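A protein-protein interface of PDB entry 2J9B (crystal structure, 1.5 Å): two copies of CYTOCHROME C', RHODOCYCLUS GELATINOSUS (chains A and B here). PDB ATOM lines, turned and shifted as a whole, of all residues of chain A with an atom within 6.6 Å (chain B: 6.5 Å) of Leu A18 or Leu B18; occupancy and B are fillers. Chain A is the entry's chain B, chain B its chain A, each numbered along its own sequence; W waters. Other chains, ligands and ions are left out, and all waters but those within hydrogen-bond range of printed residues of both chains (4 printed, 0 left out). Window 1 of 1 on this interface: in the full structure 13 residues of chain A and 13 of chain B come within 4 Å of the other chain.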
ATOM      1  N   GLU A  10     -21.078 -35.638  -7.835  1.00  0.00           N
ATOM      2  CA  GLU A  10     -20.459 -34.361  -8.130  1.00  0.00           C
ATOM      3  C   GLU A  10     -20.238 -34.200  -9.640  1.00  0.00           C
ATOM      4  O   GLU A  10     -20.416 -33.117 -10.175  1.00  0.00           O
ATOM      5  CB  GLU A  10     -19.169 -34.187  -7.349  1.00  0.00           C
ATOM      6  CG  GLU A  10     -19.485 -33.991  -5.886  1.00  0.00           C
ATOM      7  CD  GLU A  10     -18.260 -33.876  -4.986  1.00  0.00           C
ATOM      8  OE1 GLU A  10     -18.466 -33.608  -3.786  1.00  0.00           O
ATOM      9  OE2 GLU A  10     -17.101 -34.045  -5.428  1.00  0.00           O
ATOM     10  N   TYR A  11     -19.895 -35.288 -10.324  1.00  0.00           N
ATOM     11  CA  TYR A  11     -19.694 -35.236 -11.771  1.00  0.00           C
ATOM     12  C   TYR A  11     -20.975 -34.894 -12.497  1.00  0.00           C
ATOM     13  O   TYR A  11     -20.989 -34.016 -13.364  1.00  0.00           O
ATOM     14  CB  TYR A  11     -19.149 -36.566 -12.257  1.00  0.00           C
ATOM     15  CG  TYR A  11     -18.877 -36.691 -13.728  1.00  0.00           C
ATOM     16  CD1 TYR A  11     -17.623 -36.494 -14.239  1.00  0.00           C
ATOM     17  CD2 TYR A  11     -19.888 -37.094 -14.596  1.00  0.00           C
ATOM     18  CE1 TYR A  11     -17.357 -36.664 -15.602  1.00  0.00           C
ATOM     19  CE2 TYR A  11     -19.659 -37.248 -15.954  1.00  0.00           C
ATOM     20  CZ  TYR A  11     -18.392 -37.043 -16.457  1.00  0.00           C
ATOM     21  OH  TYR A  11     -18.181 -37.242 -17.796  1.00  0.00           O
ATOM     22  N   ARG A  12     -22.061 -35.602 -12.206  1.00  0.00           N
ATOM     23  CA  ARG A  12     -23.304 -35.354 -12.919  1.00  0.00           C
ATOM     24  C   ARG A  12     -23.830 -33.950 -12.645  1.00  0.00           C
ATOM     25  O   ARG A  12     -24.294 -33.257 -13.554  1.00  0.00           O
ATOM     26  CB  ARG A  12     -24.338 -36.487 -12.672  1.00  0.00           C
ATOM     27  CG  ARG A  12     -24.974 -36.534 -11.279  1.00  0.00           C
ATOM     28  CD  ARG A  12     -25.325 -37.972 -10.936  1.00  0.00           C
ATOM     29  NE  ARG A  12     -26.156 -38.046  -9.730  1.00  0.00           N
ATOM     30  CZ  ARG A  12     -26.370 -39.162  -9.047  1.00  0.00           C
ATOM     31  NH1 ARG A  12     -25.809 -40.306  -9.406  1.00  0.00           N
ATOM     32  NH2 ARG A  12     -27.192 -39.131  -8.017  1.00  0.00           N
ATOM     33  N   GLN A  13     -23.796 -33.532 -11.383  1.00  0.00           N
ATOM     34  CA  GLN A  13     -24.176 -32.170 -11.011  1.00  0.00           C
ATOM     35  C   GLN A  13     -23.372 -31.135 -11.813  1.00  0.00           C
ATOM     36  O   GLN A  13     -23.918 -30.159 -12.342  1.00  0.00           O
ATOM     37  CB  GLN A  13     -23.985 -31.969  -9.508  1.00  0.00           C
ATOM     38  CG  GLN A  13     -25.004 -32.718  -8.692  1.00  0.00           C
ATOM     39  CD  GLN A  13     -24.799 -32.547  -7.235  1.00  0.00           C
ATOM     40  OE1 GLN A  13     -23.728 -32.118  -6.785  1.00  0.00           O
ATOM     41  NE2 GLN A  13     -25.816 -32.939  -6.456  1.00  0.00           N
ATOM     42  N   SER A  14     -22.066 -31.354 -11.870  1.00  0.00           N
ATOM     43  CA  SER A  14     -21.175 -30.442 -12.582  1.00  0.00           C
ATOM     44  C   SER A  14     -21.544 -30.357 -14.077  1.00  0.00           C
ATOM     45  O   SER A  14     -21.593 -29.270 -14.643  1.00  0.00           O
ATOM     46  CB  SER A  14     -19.729 -30.884 -12.420  1.00  0.00           C
ATOM     47  OG  SER A  14     -19.291 -30.736 -11.065  1.00  0.00           O
ATOM     48  N   ALA A  15     -21.796 -31.511 -14.691  1.00  0.00           N
ATOM     49  CA  ALA A  15     -22.138 -31.502 -16.099  1.00  0.00           C
ATOM     50  C   ALA A  15     -23.460 -30.789 -16.336  1.00  0.00           C
ATOM     51  O   ALA A  15     -23.572 -30.008 -17.269  1.00  0.00           O
ATOM     52  CB  ALA A  15     -22.157 -32.923 -16.662  1.00  0.00           C
ATOM     53  N   PHE A  16     -24.467 -31.058 -15.496  1.00  0.00           N
ATOM     54  CA  PHE A  16     -25.736 -30.332 -15.605  1.00  0.00           C
ATOM     55  C   PHE A  16     -25.574 -28.815 -15.468  1.00  0.00           C
ATOM     56  O   PHE A  16     -26.192 -28.053 -16.211  1.00  0.00           O
ATOM     57  CB  PHE A  16     -26.783 -30.849 -14.614  1.00  0.00           C
ATOM     58  CG  PHE A  16     -27.332 -32.193 -14.960  1.00  0.00           C
ATOM     59  CD1 PHE A  16     -27.916 -32.410 -16.192  1.00  0.00           C
ATOM     60  CD2 PHE A  16     -27.318 -33.237 -14.046  1.00  0.00           C
ATOM     61  CE1 PHE A  16     -28.481 -33.677 -16.511  1.00  0.00           C
ATOM     62  CE2 PHE A  16     -27.879 -34.486 -14.380  1.00  0.00           C
ATOM     63  CZ  PHE A  16     -28.435 -34.684 -15.585  1.00  0.00           C
ATOM     64  N   THR A  17     -24.740 -28.373 -14.533  1.00  0.00           N
ATOM     65  CA  THR A  17     -24.468 -26.940 -14.373  1.00  0.00           C
ATOM     66  C   THR A  17     -23.909 -26.327 -15.663  1.00  0.00           C
ATOM     67  O   THR A  17     -24.374 -25.284 -16.108  1.00  0.00           O
ATOM     68  CB  THR A  17     -23.534 -26.697 -13.202  1.00  0.00           C
ATOM     69  OG1 THR A  17     -24.240 -27.046 -11.996  1.00  0.00           O
ATOM     70  CG2 THR A  17     -23.082 -25.239 -13.148  1.00  0.00           C
ATOM     71  N   LEU A  18     -22.934 -26.994 -16.271  1.00  0.00           N
ATOM     72  CA  LEU A  18     -22.348 -26.449 -17.504  1.00  0.00           C
ATOM     73  C   LEU A  18     -23.347 -26.487 -18.665  1.00  0.00           C
ATOM     74  O   LEU A  18     -23.413 -25.546 -19.444  1.00  0.00           O
ATOM     75  CB  LEU A  18     -21.089 -27.214 -17.888  1.00  0.00           C
ATOM     76  CG  LEU A  18     -19.940 -27.163 -16.859  1.00  0.00           C
ATOM     77  CD1 LEU A  18     -18.732 -27.896 -17.467  1.00  0.00           C
ATOM     78  CD2 LEU A  18     -19.578 -25.758 -16.553  1.00  0.00           C
ATOM     79  N   ILE A  19     -24.115 -27.566 -18.754  1.00  0.00           N
ATOM     80  CA  ILE A  19     -25.191 -27.671 -19.757  1.00  0.00           C
ATOM     81  C   ILE A  19     -26.144 -26.493 -19.597  1.00  0.00           C
ATOM     82  O   ILE A  19     -26.494 -25.834 -20.577  1.00  0.00           O
ATOM     83  CB  ILE A  19     -25.935 -29.038 -19.681  1.00  0.00           C
ATOM     84  CG1 ILE A  19     -25.046 -30.200 -20.112  1.00  0.00           C
ATOM     85  CG2 ILE A  19     -27.224 -29.022 -20.503  1.00  0.00           C
ATOM     86  CD1 ILE A  19     -25.519 -31.585 -19.703  1.00  0.00           C
ATOM     87  N   ALA A  20     -26.604 -26.257 -18.376  1.00  0.00           N
ATOM     88  CA  ALA A  20     -27.571 -25.198 -18.140  1.00  0.00           C
ATOM     89  C   ALA A  20     -27.017 -23.838 -18.546  1.00  0.00           C
ATOM     90  O   ALA A  20     -27.713 -23.012 -19.151  1.00  0.00           O
ATOM     91  CB  ALA A  20     -27.990 -25.164 -16.701  1.00  0.00           C
ATOM     92  N   ASN A  21     -25.748 -23.583 -18.249  1.00  0.00           N
ATOM     93  CA  ASN A  21     -25.187 -22.284 -18.606  1.00  0.00           C
ATOM     94  C   ASN A  21     -25.100 -22.089 -20.110  1.00  0.00           C
ATOM     95  O   ASN A  21     -25.567 -21.092 -20.632  1.00  0.00           O
ATOM     96  CB  ASN A  21     -23.842 -22.047 -17.955  1.00  0.00           C
ATOM     97  CG  ASN A  21     -23.312 -20.689 -18.259  1.00  0.00           C
ATOM     98  OD1 ASN A  21     -22.686 -20.493 -19.299  1.00  0.00           O
ATOM     99  ND2 ASN A  21     -23.596 -19.701 -17.381  1.00  0.00           N
ATOM    100  N   HIS A  22     -24.533 -23.062 -20.797  1.00  0.00           N
ATOM    101  CA  HIS A  22     -24.383 -22.908 -22.239  1.00  0.00           C
ATOM    102  C   HIS A  22     -25.708 -22.949 -22.980  1.00  0.00           C
ATOM    103  O   HIS A  22     -25.907 -22.201 -23.929  1.00  0.00           O
ATOM    104  CB  HIS A  22     -23.338 -23.899 -22.774  1.00  0.00           C
ATOM    105  CG  HIS A  22     -21.957 -23.498 -22.361  1.00  0.00           C
ATOM    106  ND1 HIS A  22     -21.275 -22.502 -23.020  1.00  0.00           N
ATOM    107  CD2 HIS A  22     -21.199 -23.837 -21.292  1.00  0.00           C
ATOM    108  CE1 HIS A  22     -20.131 -22.274 -22.381  1.00  0.00           C
ATOM    109  NE2 HIS A  22     -20.075 -23.057 -21.328  1.00  0.00           N
ATOM    110  N   PHE A  23     -26.613 -23.822 -22.550  1.00  0.00           N
ATOM    111  CA  PHE A  23     -27.966 -23.855 -23.125  1.00  0.00           C
ATOM    112  C   PHE A  23     -28.657 -22.508 -22.921  1.00  0.00           C
ATOM    113  O   PHE A  23     -29.317 -21.992 -23.817  1.00  0.00           O
ATOM    114  CB  PHE A  23     -28.780 -25.012 -22.540  1.00  0.00           C
ATOM    115  CG  PHE A  23     -30.152 -25.130 -23.105  1.00  0.00           C
ATOM    116  CD1 PHE A  23     -30.326 -25.452 -24.427  1.00  0.00           C
ATOM    117  CD2 PHE A  23     -31.262 -24.935 -22.317  1.00  0.00           C
ATOM    118  CE1 PHE A  23     -31.589 -25.533 -24.971  1.00  0.00           C
ATOM    119  CE2 PHE A  23     -32.528 -25.018 -22.856  1.00  0.00           C
ATOM    120  CZ  PHE A  23     -32.676 -25.351 -24.185  1.00  0.00           C
ATOM    121  N   VAL A  48     -23.126 -27.786 -25.557  1.00  0.00           N
ATOM    122  CA  VAL A  48     -24.251 -28.509 -24.996  1.00  0.00           C
ATOM    123  C   VAL A  48     -24.277 -29.941 -25.508  1.00  0.00           C
ATOM    124  O   VAL A  48     -24.479 -30.864 -24.721  1.00  0.00           O
ATOM    125  CB  VAL A  48     -25.601 -27.779 -25.241  1.00  0.00           C
ATOM    126  CG1 VAL A  48     -26.797 -28.666 -24.925  1.00  0.00           C
ATOM    127  CG2 VAL A  48     -25.626 -26.436 -24.516  1.00  0.00           C
ATOM    128  N   LEU A  51     -21.466 -31.947 -23.836  1.00  0.00           N
ATOM    129  CA  LEU A  51     -21.726 -32.120 -22.415  1.00  0.00           C
ATOM    130  C   LEU A  51     -22.904 -33.043 -22.161  1.00  0.00           C
ATOM    131  O   LEU A  51     -22.941 -33.747 -21.152  1.00  0.00           O
ATOM    132  CB  LEU A  51     -21.953 -30.755 -21.751  1.00  0.00           C
ATOM    133  CG  LEU A  51     -20.756 -29.804 -21.679  1.00  0.00           C
ATOM    134  CD1 LEU A  51     -21.249 -28.361 -21.398  1.00  0.00           C
ATOM    135  CD2 LEU A  51     -19.773 -30.280 -20.615  1.00  0.00           C
ATOM    136  N   LEU A  54     -22.575 -36.683 -21.036  1.00  0.00           N
ATOM    137  CA  LEU A  54     -21.836 -36.993 -19.810  1.00  0.00           C
ATOM    138  C   LEU A  54     -22.652 -37.342 -18.539  1.00  0.00           C
ATOM    139  O   LEU A  54     -22.375 -38.354 -17.886  1.00  0.00           O
ATOM    140  CB  LEU A  54     -20.864 -35.867 -19.523  1.00  0.00           C
ATOM    141  CG  LEU A  54     -19.910 -35.450 -20.626  1.00  0.00           C
ATOM    142  CD1 LEU A  54     -19.005 -34.340 -20.135  1.00  0.00           C
ATOM    143  CD2 LEU A  54     -19.127 -36.626 -21.168  1.00  0.00           C
ATOM    144  N   GLU B  10     -20.009 -21.541  -9.334  1.00  0.00           N
ATOM    145  CA  GLU B  10     -20.477 -22.907  -9.548  1.00  0.00           C
ATOM    146  C   GLU B  10     -20.003 -23.433 -10.908  1.00  0.00           C
ATOM    147  O   GLU B  10     -19.708 -24.611 -11.063  1.00  0.00           O
ATOM    148  CB  GLU B  10     -21.990 -23.001  -9.450  1.00  0.00           C
ATOM    149  CG  GLU B  10     -22.606 -22.763  -8.088  1.00  0.00           C
ATOM    150  CD  GLU B  10     -24.106 -23.068  -8.133  1.00  0.00           C
ATOM    151  OE1 GLU B  10     -24.455 -24.255  -8.257  1.00  0.00           O
ATOM    152  OE2 GLU B  10     -24.931 -22.142  -8.094  1.00  0.00           O
ATOM    153  N   TYR B  11     -19.985 -22.566 -11.909  1.00  0.00           N
ATOM    154  CA  TYR B  11     -19.553 -22.918 -13.268  1.00  0.00           C
ATOM    155  C   TYR B  11     -18.104 -23.339 -13.274  1.00  0.00           C
ATOM    156  O   TYR B  11     -17.760 -24.409 -13.798  1.00  0.00           O
ATOM    157  CB  TYR B  11     -19.768 -21.738 -14.207  1.00  0.00           C
ATOM    158  CG  TYR B  11     -19.366 -21.936 -15.638  1.00  0.00           C
ATOM    159  CD1 TYR B  11     -20.297 -22.326 -16.598  1.00  0.00           C
ATOM    160  CD2 TYR B  11     -18.066 -21.700 -16.051  1.00  0.00           C
ATOM    161  CE1 TYR B  11     -19.917 -22.449 -17.939  1.00  0.00           C
ATOM    162  CE2 TYR B  11     -17.683 -21.848 -17.383  1.00  0.00           C
ATOM    163  CZ  TYR B  11     -18.606 -22.213 -18.313  1.00  0.00           C
ATOM    164  OH  TYR B  11     -18.169 -22.339 -19.603  1.00  0.00           O
ATOM    165  N   ARG B  12     -17.210 -22.546 -12.681  1.00  0.00           N
ATOM    166  CA  ARG B  12     -15.798 -22.888 -12.748  1.00  0.00           C
ATOM    167  C   ARG B  12     -15.522 -24.151 -11.953  1.00  0.00           C
ATOM    168  O   ARG B  12     -14.749 -25.004 -12.399  1.00  0.00           O
ATOM    169  CB  ARG B  12     -14.901 -21.702 -12.336  1.00  0.00           C
ATOM    170  CG  ARG B  12     -14.921 -21.332 -10.860  1.00  0.00           C
ATOM    171  CD  ARG B  12     -14.645 -19.864 -10.685  1.00  0.00           C
ATOM    172  NE  ARG B  12     -14.490 -19.509  -9.270  1.00  0.00           N
ATOM    173  CZ  ARG B  12     -14.557 -18.258  -8.834  1.00  0.00           C
ATOM    174  NH1 ARG B  12     -14.820 -17.258  -9.663  1.00  0.00           N
ATOM    175  NH2 ARG B  12     -14.335 -17.994  -7.557  1.00  0.00           N
ATOM    176  N   GLN B  13     -16.117 -24.288 -10.774  1.00  0.00           N
ATOM    177  CA  GLN B  13     -15.981 -25.506  -9.977  1.00  0.00           C
ATOM    178  C   GLN B  13     -16.412 -26.731 -10.783  1.00  0.00           C
ATOM    179  O   GLN B  13     -15.723 -27.770 -10.792  1.00  0.00           O
ATOM    180  CB  GLN B  13     -16.817 -25.393  -8.709  1.00  0.00           C
ATOM    181  CG  GLN B  13     -16.222 -24.403  -7.696  1.00  0.00           C
ATOM    182  CD  GLN B  13     -17.105 -24.104  -6.540  1.00  0.00           C
ATOM    183  OE1 GLN B  13     -18.309 -24.470  -6.527  1.00  0.00           O
ATOM    184  NE2 GLN B  13     -16.514 -23.510  -5.529  1.00  0.00           N
ATOM    185  N   SER B  14     -17.563 -26.611 -11.431  1.00  0.00           N
ATOM    186  CA  SER B  14     -18.104 -27.699 -12.244  1.00  0.00           C
ATOM    187  C   SER B  14     -17.146 -28.089 -13.382  1.00  0.00           C
ATOM    188  O   SER B  14     -16.904 -29.293 -13.633  1.00  0.00           O
ATOM    189  CB  SER B  14     -19.465 -27.275 -12.805  1.00  0.00           C
ATOM    190  OG  SER B  14     -20.442 -27.175 -11.769  1.00  0.00           O
ATOM    191  N   ALA B  15     -16.619 -27.084 -14.079  1.00  0.00           N
ATOM    192  CA  ALA B  15     -15.683 -27.378 -15.164  1.00  0.00           C
ATOM    193  C   ALA B  15     -14.438 -28.058 -14.648  1.00  0.00           C
ATOM    194  O   ALA B  15     -13.970 -29.024 -15.251  1.00  0.00           O
ATOM    195  CB  ALA B  15     -15.335 -26.133 -15.954  1.00  0.00           C
ATOM    196  N   PHE B  16     -13.894 -27.585 -13.528  1.00  0.00           N
ATOM    197  CA  PHE B  16     -12.721 -28.214 -12.950  1.00  0.00           C
ATOM    198  C   PHE B  16     -12.992 -29.668 -12.575  1.00  0.00           C
ATOM    199  O   PHE B  16     -12.145 -30.518 -12.760  1.00  0.00           O
ATOM    200  CB  PHE B  16     -12.197 -27.436 -11.749  1.00  0.00           C
ATOM    201  CG  PHE B  16     -11.451 -26.163 -12.107  1.00  0.00           C
ATOM    202  CD1 PHE B  16     -10.371 -26.172 -12.967  1.00  0.00           C
ATOM    203  CD2 PHE B  16     -11.832 -24.960 -11.517  1.00  0.00           C
ATOM    204  CE1 PHE B  16      -9.677 -25.008 -13.255  1.00  0.00           C
ATOM    205  CE2 PHE B  16     -11.150 -23.812 -11.790  1.00  0.00           C
ATOM    206  CZ  PHE B  16     -10.091 -23.823 -12.648  1.00  0.00           C
ATOM    207  N   THR B  17     -14.157 -29.952 -12.006  1.00  0.00           N
ATOM    208  CA  THR B  17     -14.521 -31.328 -11.659  1.00  0.00           C
ATOM    209  C   THR B  17     -14.531 -32.216 -12.889  1.00  0.00           C
ATOM    210  O   THR B  17     -13.962 -33.297 -12.882  1.00  0.00           O
ATOM    211  CB  THR B  17     -15.861 -31.371 -10.945  1.00  0.00           C
ATOM    212  OG1 THR B  17     -15.747 -30.748  -9.666  1.00  0.00           O
ATOM    213  CG2 THR B  17     -16.377 -32.794 -10.794  1.00  0.00           C
ATOM    214  N   LEU B  18     -15.127 -31.747 -13.984  1.00  0.00           N
ATOM    215  CA  LEU B  18     -15.143 -32.574 -15.193  1.00  0.00           C
ATOM    216  C   LEU B  18     -13.734 -32.745 -15.781  1.00  0.00           C
ATOM    217  O   LEU B  18     -13.365 -33.832 -16.254  1.00  0.00           O
ATOM    218  CB  LEU B  18     -16.097 -31.990 -16.232  1.00  0.00           C
ATOM    219  CG  LEU B  18     -17.590 -31.870 -15.841  1.00  0.00           C
ATOM    220  CD1 LEU B  18     -18.394 -31.420 -17.044  1.00  0.00           C
ATOM    221  CD2 LEU B  18     -18.139 -33.140 -15.328  1.00  0.00           C
ATOM    222  N   ILE B  19     -12.952 -31.665 -15.776  1.00  0.00           N
ATOM    223  CA  ILE B  19     -11.561 -31.719 -16.241  1.00  0.00           C
ATOM    224  C   ILE B  19     -10.800 -32.767 -15.432  1.00  0.00           C
ATOM    225  O   ILE B  19     -10.085 -33.623 -15.993  1.00  0.00           O
ATOM    226  CB  ILE B  19     -10.853 -30.334 -16.127  1.00  0.00           C
ATOM    227  CG1 ILE B  19     -11.435 -29.368 -17.164  1.00  0.00           C
ATOM    228  CG2 ILE B  19      -9.355 -30.475 -16.294  1.00  0.00           C
ATOM    229  CD1 ILE B  19     -11.130 -27.916 -16.893  1.00  0.00           C
ATOM    230  N   ALA B  20     -10.937 -32.706 -14.111  1.00  0.00           N
ATOM    231  CA  ALA B  20     -10.173 -33.639 -13.258  1.00  0.00           C
ATOM    232  C   ALA B  20     -10.554 -35.080 -13.554  1.00  0.00           C
ATOM    233  O   ALA B  20      -9.697 -35.972 -13.612  1.00  0.00           O
ATOM    234  CB  ALA B  20     -10.403 -33.318 -11.764  1.00  0.00           C
ATOM    235  N   ASN B  21     -11.843 -35.330 -13.775  1.00  0.00           N
ATOM    236  CA  ASN B  21     -12.274 -36.701 -14.031  1.00  0.00           C
ATOM    237  C   ASN B  21     -11.706 -37.228 -15.346  1.00  0.00           C
ATOM    238  O   ASN B  21     -11.105 -38.302 -15.418  1.00  0.00           O
ATOM    239  CB  ASN B  21     -13.799 -36.821 -14.016  1.00  0.00           C
ATOM    240  CG  ASN B  21     -14.234 -38.238 -14.175  1.00  0.00           C
ATOM    241  OD1 ASN B  21     -14.291 -38.734 -15.287  1.00  0.00           O
ATOM    242  ND2 ASN B  21     -14.492 -38.920 -13.040  1.00  0.00           N
ATOM    243  N   HIS B  22     -11.860 -36.465 -16.405  1.00  0.00           N
ATOM    244  CA  HIS B  22     -11.415 -36.956 -17.705  1.00  0.00           C
ATOM    245  C   HIS B  22      -9.892 -36.969 -17.831  1.00  0.00           C
ATOM    246  O   HIS B  22      -9.317 -37.888 -18.407  1.00  0.00           O
ATOM    247  CB  HIS B  22     -12.119 -36.173 -18.812  1.00  0.00           C
ATOM    248  CG  HIS B  22     -13.557 -36.572 -18.941  1.00  0.00           C
ATOM    249  ND1 HIS B  22     -13.943 -37.747 -19.555  1.00  0.00           N
ATOM    250  CD2 HIS B  22     -14.681 -36.055 -18.375  1.00  0.00           C
ATOM    251  CE1 HIS B  22     -15.247 -37.911 -19.389  1.00  0.00           C
ATOM    252  NE2 HIS B  22     -15.722 -36.886 -18.697  1.00  0.00           N
ATOM    253  N   PHE B  23      -9.223 -35.978 -17.245  1.00  0.00           N
ATOM    254  CA  PHE B  23      -7.770 -35.980 -17.207  1.00  0.00           C
ATOM    255  C   PHE B  23      -7.268 -37.173 -16.410  1.00  0.00           C
ATOM    256  O   PHE B  23      -6.293 -37.821 -16.804  1.00  0.00           O
ATOM    257  CB  PHE B  23      -7.251 -34.675 -16.587  1.00  0.00           C
ATOM    258  CG  PHE B  23      -5.745 -34.580 -16.571  1.00  0.00           C
ATOM    259  CD1 PHE B  23      -5.030 -34.507 -17.744  1.00  0.00           C
ATOM    260  CD2 PHE B  23      -5.061 -34.545 -15.389  1.00  0.00           C
ATOM    261  CE1 PHE B  23      -3.678 -34.442 -17.758  1.00  0.00           C
ATOM    262  CE2 PHE B  23      -3.691 -34.493 -15.389  1.00  0.00           C
ATOM    263  CZ  PHE B  23      -3.015 -34.420 -16.542  1.00  0.00           C
ATOM    264  N   VAL B  48     -10.934 -33.017 -22.298  1.00  0.00           N
ATOM    265  CA  VAL B  48     -10.123 -32.147 -21.445  1.00  0.00           C
ATOM    266  C   VAL B  48      -9.799 -30.859 -22.198  1.00  0.00           C
ATOM    267  O   VAL B  48      -9.894 -29.766 -21.630  1.00  0.00           O
ATOM    268  CB  VAL B  48      -8.820 -32.863 -20.980  1.00  0.00           C
ATOM    269  CG1 VAL B  48      -7.835 -31.869 -20.373  1.00  0.00           C
ATOM    270  CG2 VAL B  48      -9.129 -34.026 -20.028  1.00  0.00           C
ATOM    271  N   LEU B  51     -12.963 -28.657 -22.345  1.00  0.00           N
ATOM    272  CA  LEU B  51     -13.334 -28.156 -21.024  1.00  0.00           C
ATOM    273  C   LEU B  51     -12.335 -27.155 -20.487  1.00  0.00           C
ATOM    274  O   LEU B  51     -12.709 -26.264 -19.723  1.00  0.00           O
ATOM    275  CB  LEU B  51     -13.474 -29.340 -20.061  1.00  0.00           C
ATOM    276  CG  LEU B  51     -14.615 -30.337 -20.281  1.00  0.00           C
ATOM    277  CD1 LEU B  51     -14.349 -31.634 -19.538  1.00  0.00           C
ATOM    278  CD2 LEU B  51     -15.940 -29.718 -19.830  1.00  0.00           C
ATOM    279  N   LEU B  54     -12.925 -23.419 -20.501  1.00  0.00           N
ATOM    280  CA  LEU B  54     -14.078 -22.865 -19.794  1.00  0.00           C
ATOM    281  C   LEU B  54     -13.832 -22.216 -18.402  1.00  0.00           C
ATOM    282  O   LEU B  54     -14.317 -21.116 -18.156  1.00  0.00           O
ATOM    283  CB  LEU B  54     -15.152 -23.956 -19.657  1.00  0.00           C
ATOM    284  CG  LEU B  54     -15.583 -24.711 -20.913  1.00  0.00           C
ATOM    285  CD1 LEU B  54     -16.707 -25.685 -20.604  1.00  0.00           C
ATOM    286  CD2 LEU B  54     -15.967 -23.699 -21.993  1.00  0.00           C
HETATM  287  O   HOH W   1     -17.606 -29.366  -8.486  1.00  0.00           O
HETATM  288  O   HOH W   2     -20.289 -28.514  -9.143  1.00  0.00           O
HETATM  289  O   HOH W   3     -23.128 -28.171  -9.842  1.00  0.00           O
HETATM  290  O   HOH W   4     -26.068 -25.075 -11.133  1.00  0.00           O
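A ring nitrogen (NE2) of His A22 is in hydrogen-bond range of the side-chain hydroxyl of Tyr B11 (2.7 Å).
OH of Tyr A11 sits at hydrogen-bond distance from NE2 of His B22, 2.6 Å away.
OG of Ser B14 is in hydrogen-bond range of O of Glu B10, 2.8 Å away.
The backbone carbonyl oxygen (O) of Gln B13 sits at hydrogen-bond distance from the side-chain hydroxyl (OG1) of Thr B17 (3.2 Å).
The backbone carbonyl oxygen (O) of Glu A10 is in hydrogen-bond range of the side-chain hydroxyl (OG) of Ser A14, at 2.8 Å.
The side-chain hydroxyl (OG1) of Thr A17 is in hydrogen-bond range of the backbone carbonyl oxygen (O) of Gln A13 (3.1 Å).
Among the printed residues, merely in contact across the chains: Tyr A11 with Leu B18 (3.6 Å), Tyr A11 with Asn B21 (3.7 Å), Ser A14 with Ser B14 (3.4 Å), Ser A14 with Thr B17 (3.5 Å), Ala A15 with Leu B18 (3.9 Å), Thr A17 with Ser B14 (3.4 Å), Leu A18 with Tyr B11 (3.5 Å), Leu A18 with Ala B15 (3.9 Å), Leu A18 with Leu B18 (3.6 Å), Asn A21 with Tyr B11 (3.7 Å), Leu A51 with Leu B18 (3.99 Å) and Leu A51 with Leu B51 (3.95 Å).
Printed residues of chain B within 4 Å of Tyr A11: Leu B18, Asn B21 and His B22.
Leu A18 touches just these residues of chain B: Tyr B11 (3.5 Å), Ala B15 (3.9 Å) and Leu B18 (3.6 Å).
Ile A19 touches none of the printed residues of chain B.
Of the printed residues of chain A, Thr B17 touches Ser A14.
Ala B20 touches none of the printed residues of chain A.
The nearest printed residue of chain B that does not touch His A22 is Leu B54 (4.2 Å).
Printed residues of chain B that touch a printed residue of chain A: Tyr B11, Ser B14, Ala B15, Thr B17, Leu B18, Asn B21, His B22 and Leu B51.
Hydrophobic or aromatic side chains of chain B that line the printed part of chain A: Tyr B11, Leu B18, His B22 and Leu B51.
Of the 17 printed residues of chain A, 8 touch a printed residue of chain B.
Hydrophobic or aromatic side chains of chain A that line the printed part of chain B: Tyr A11, Leu A18, His A22 and Leu A51.
Along chain A the printed residues that touch a printed residue of chain B span positions 11 to 51.
Among the printed residues, 14 pairs touch across the chains.
Ser A14 touches Thr B17, and with the chains exchanged Thr A17 touches Ser B14.
Ala A15 touches Leu B18, and with the chains exchanged Leu A18 touches Ala B15.
Leu A18 touches its own counterpart, Leu B18.
Leu A51 touches Leu B18, but with the chains exchanged Leu A18 does not touch Leu B51 (4.1 Å).
Positions printed for both chains: 10, 11, 12, 13, 14, 15, 16, 17, 18, 19, 20, 21, 22, 23, 48, 51 and 54.
Water W1 lies within hydrogen-bond range of the side-chain hydroxyl (OG1) of Thr B17 (2.6 Å), the side-chain hydroxyl (OG) of Ser A14 (3.4 Å) and the backbone carbonyl oxygen (O) of Gln B13 (3.4 Å).
Water W3 lies within hydrogen-bond range of OG1 of Thr A17 (2.7 Å), O of Gln A13 (3.3 Å) and OG of Ser B14 (3.5 Å).
Water W4 bridges the side-chain hydroxyl (OG1) of Thr A17 (2.8 Å) and the side-chain carboxylate (OE1) of Glu B10 (3.4 Å).
Water W2 lies within hydrogen-bond range of OG of Ser B14 (3.0 Å) and OG of Ser A14 (3.1 Å).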
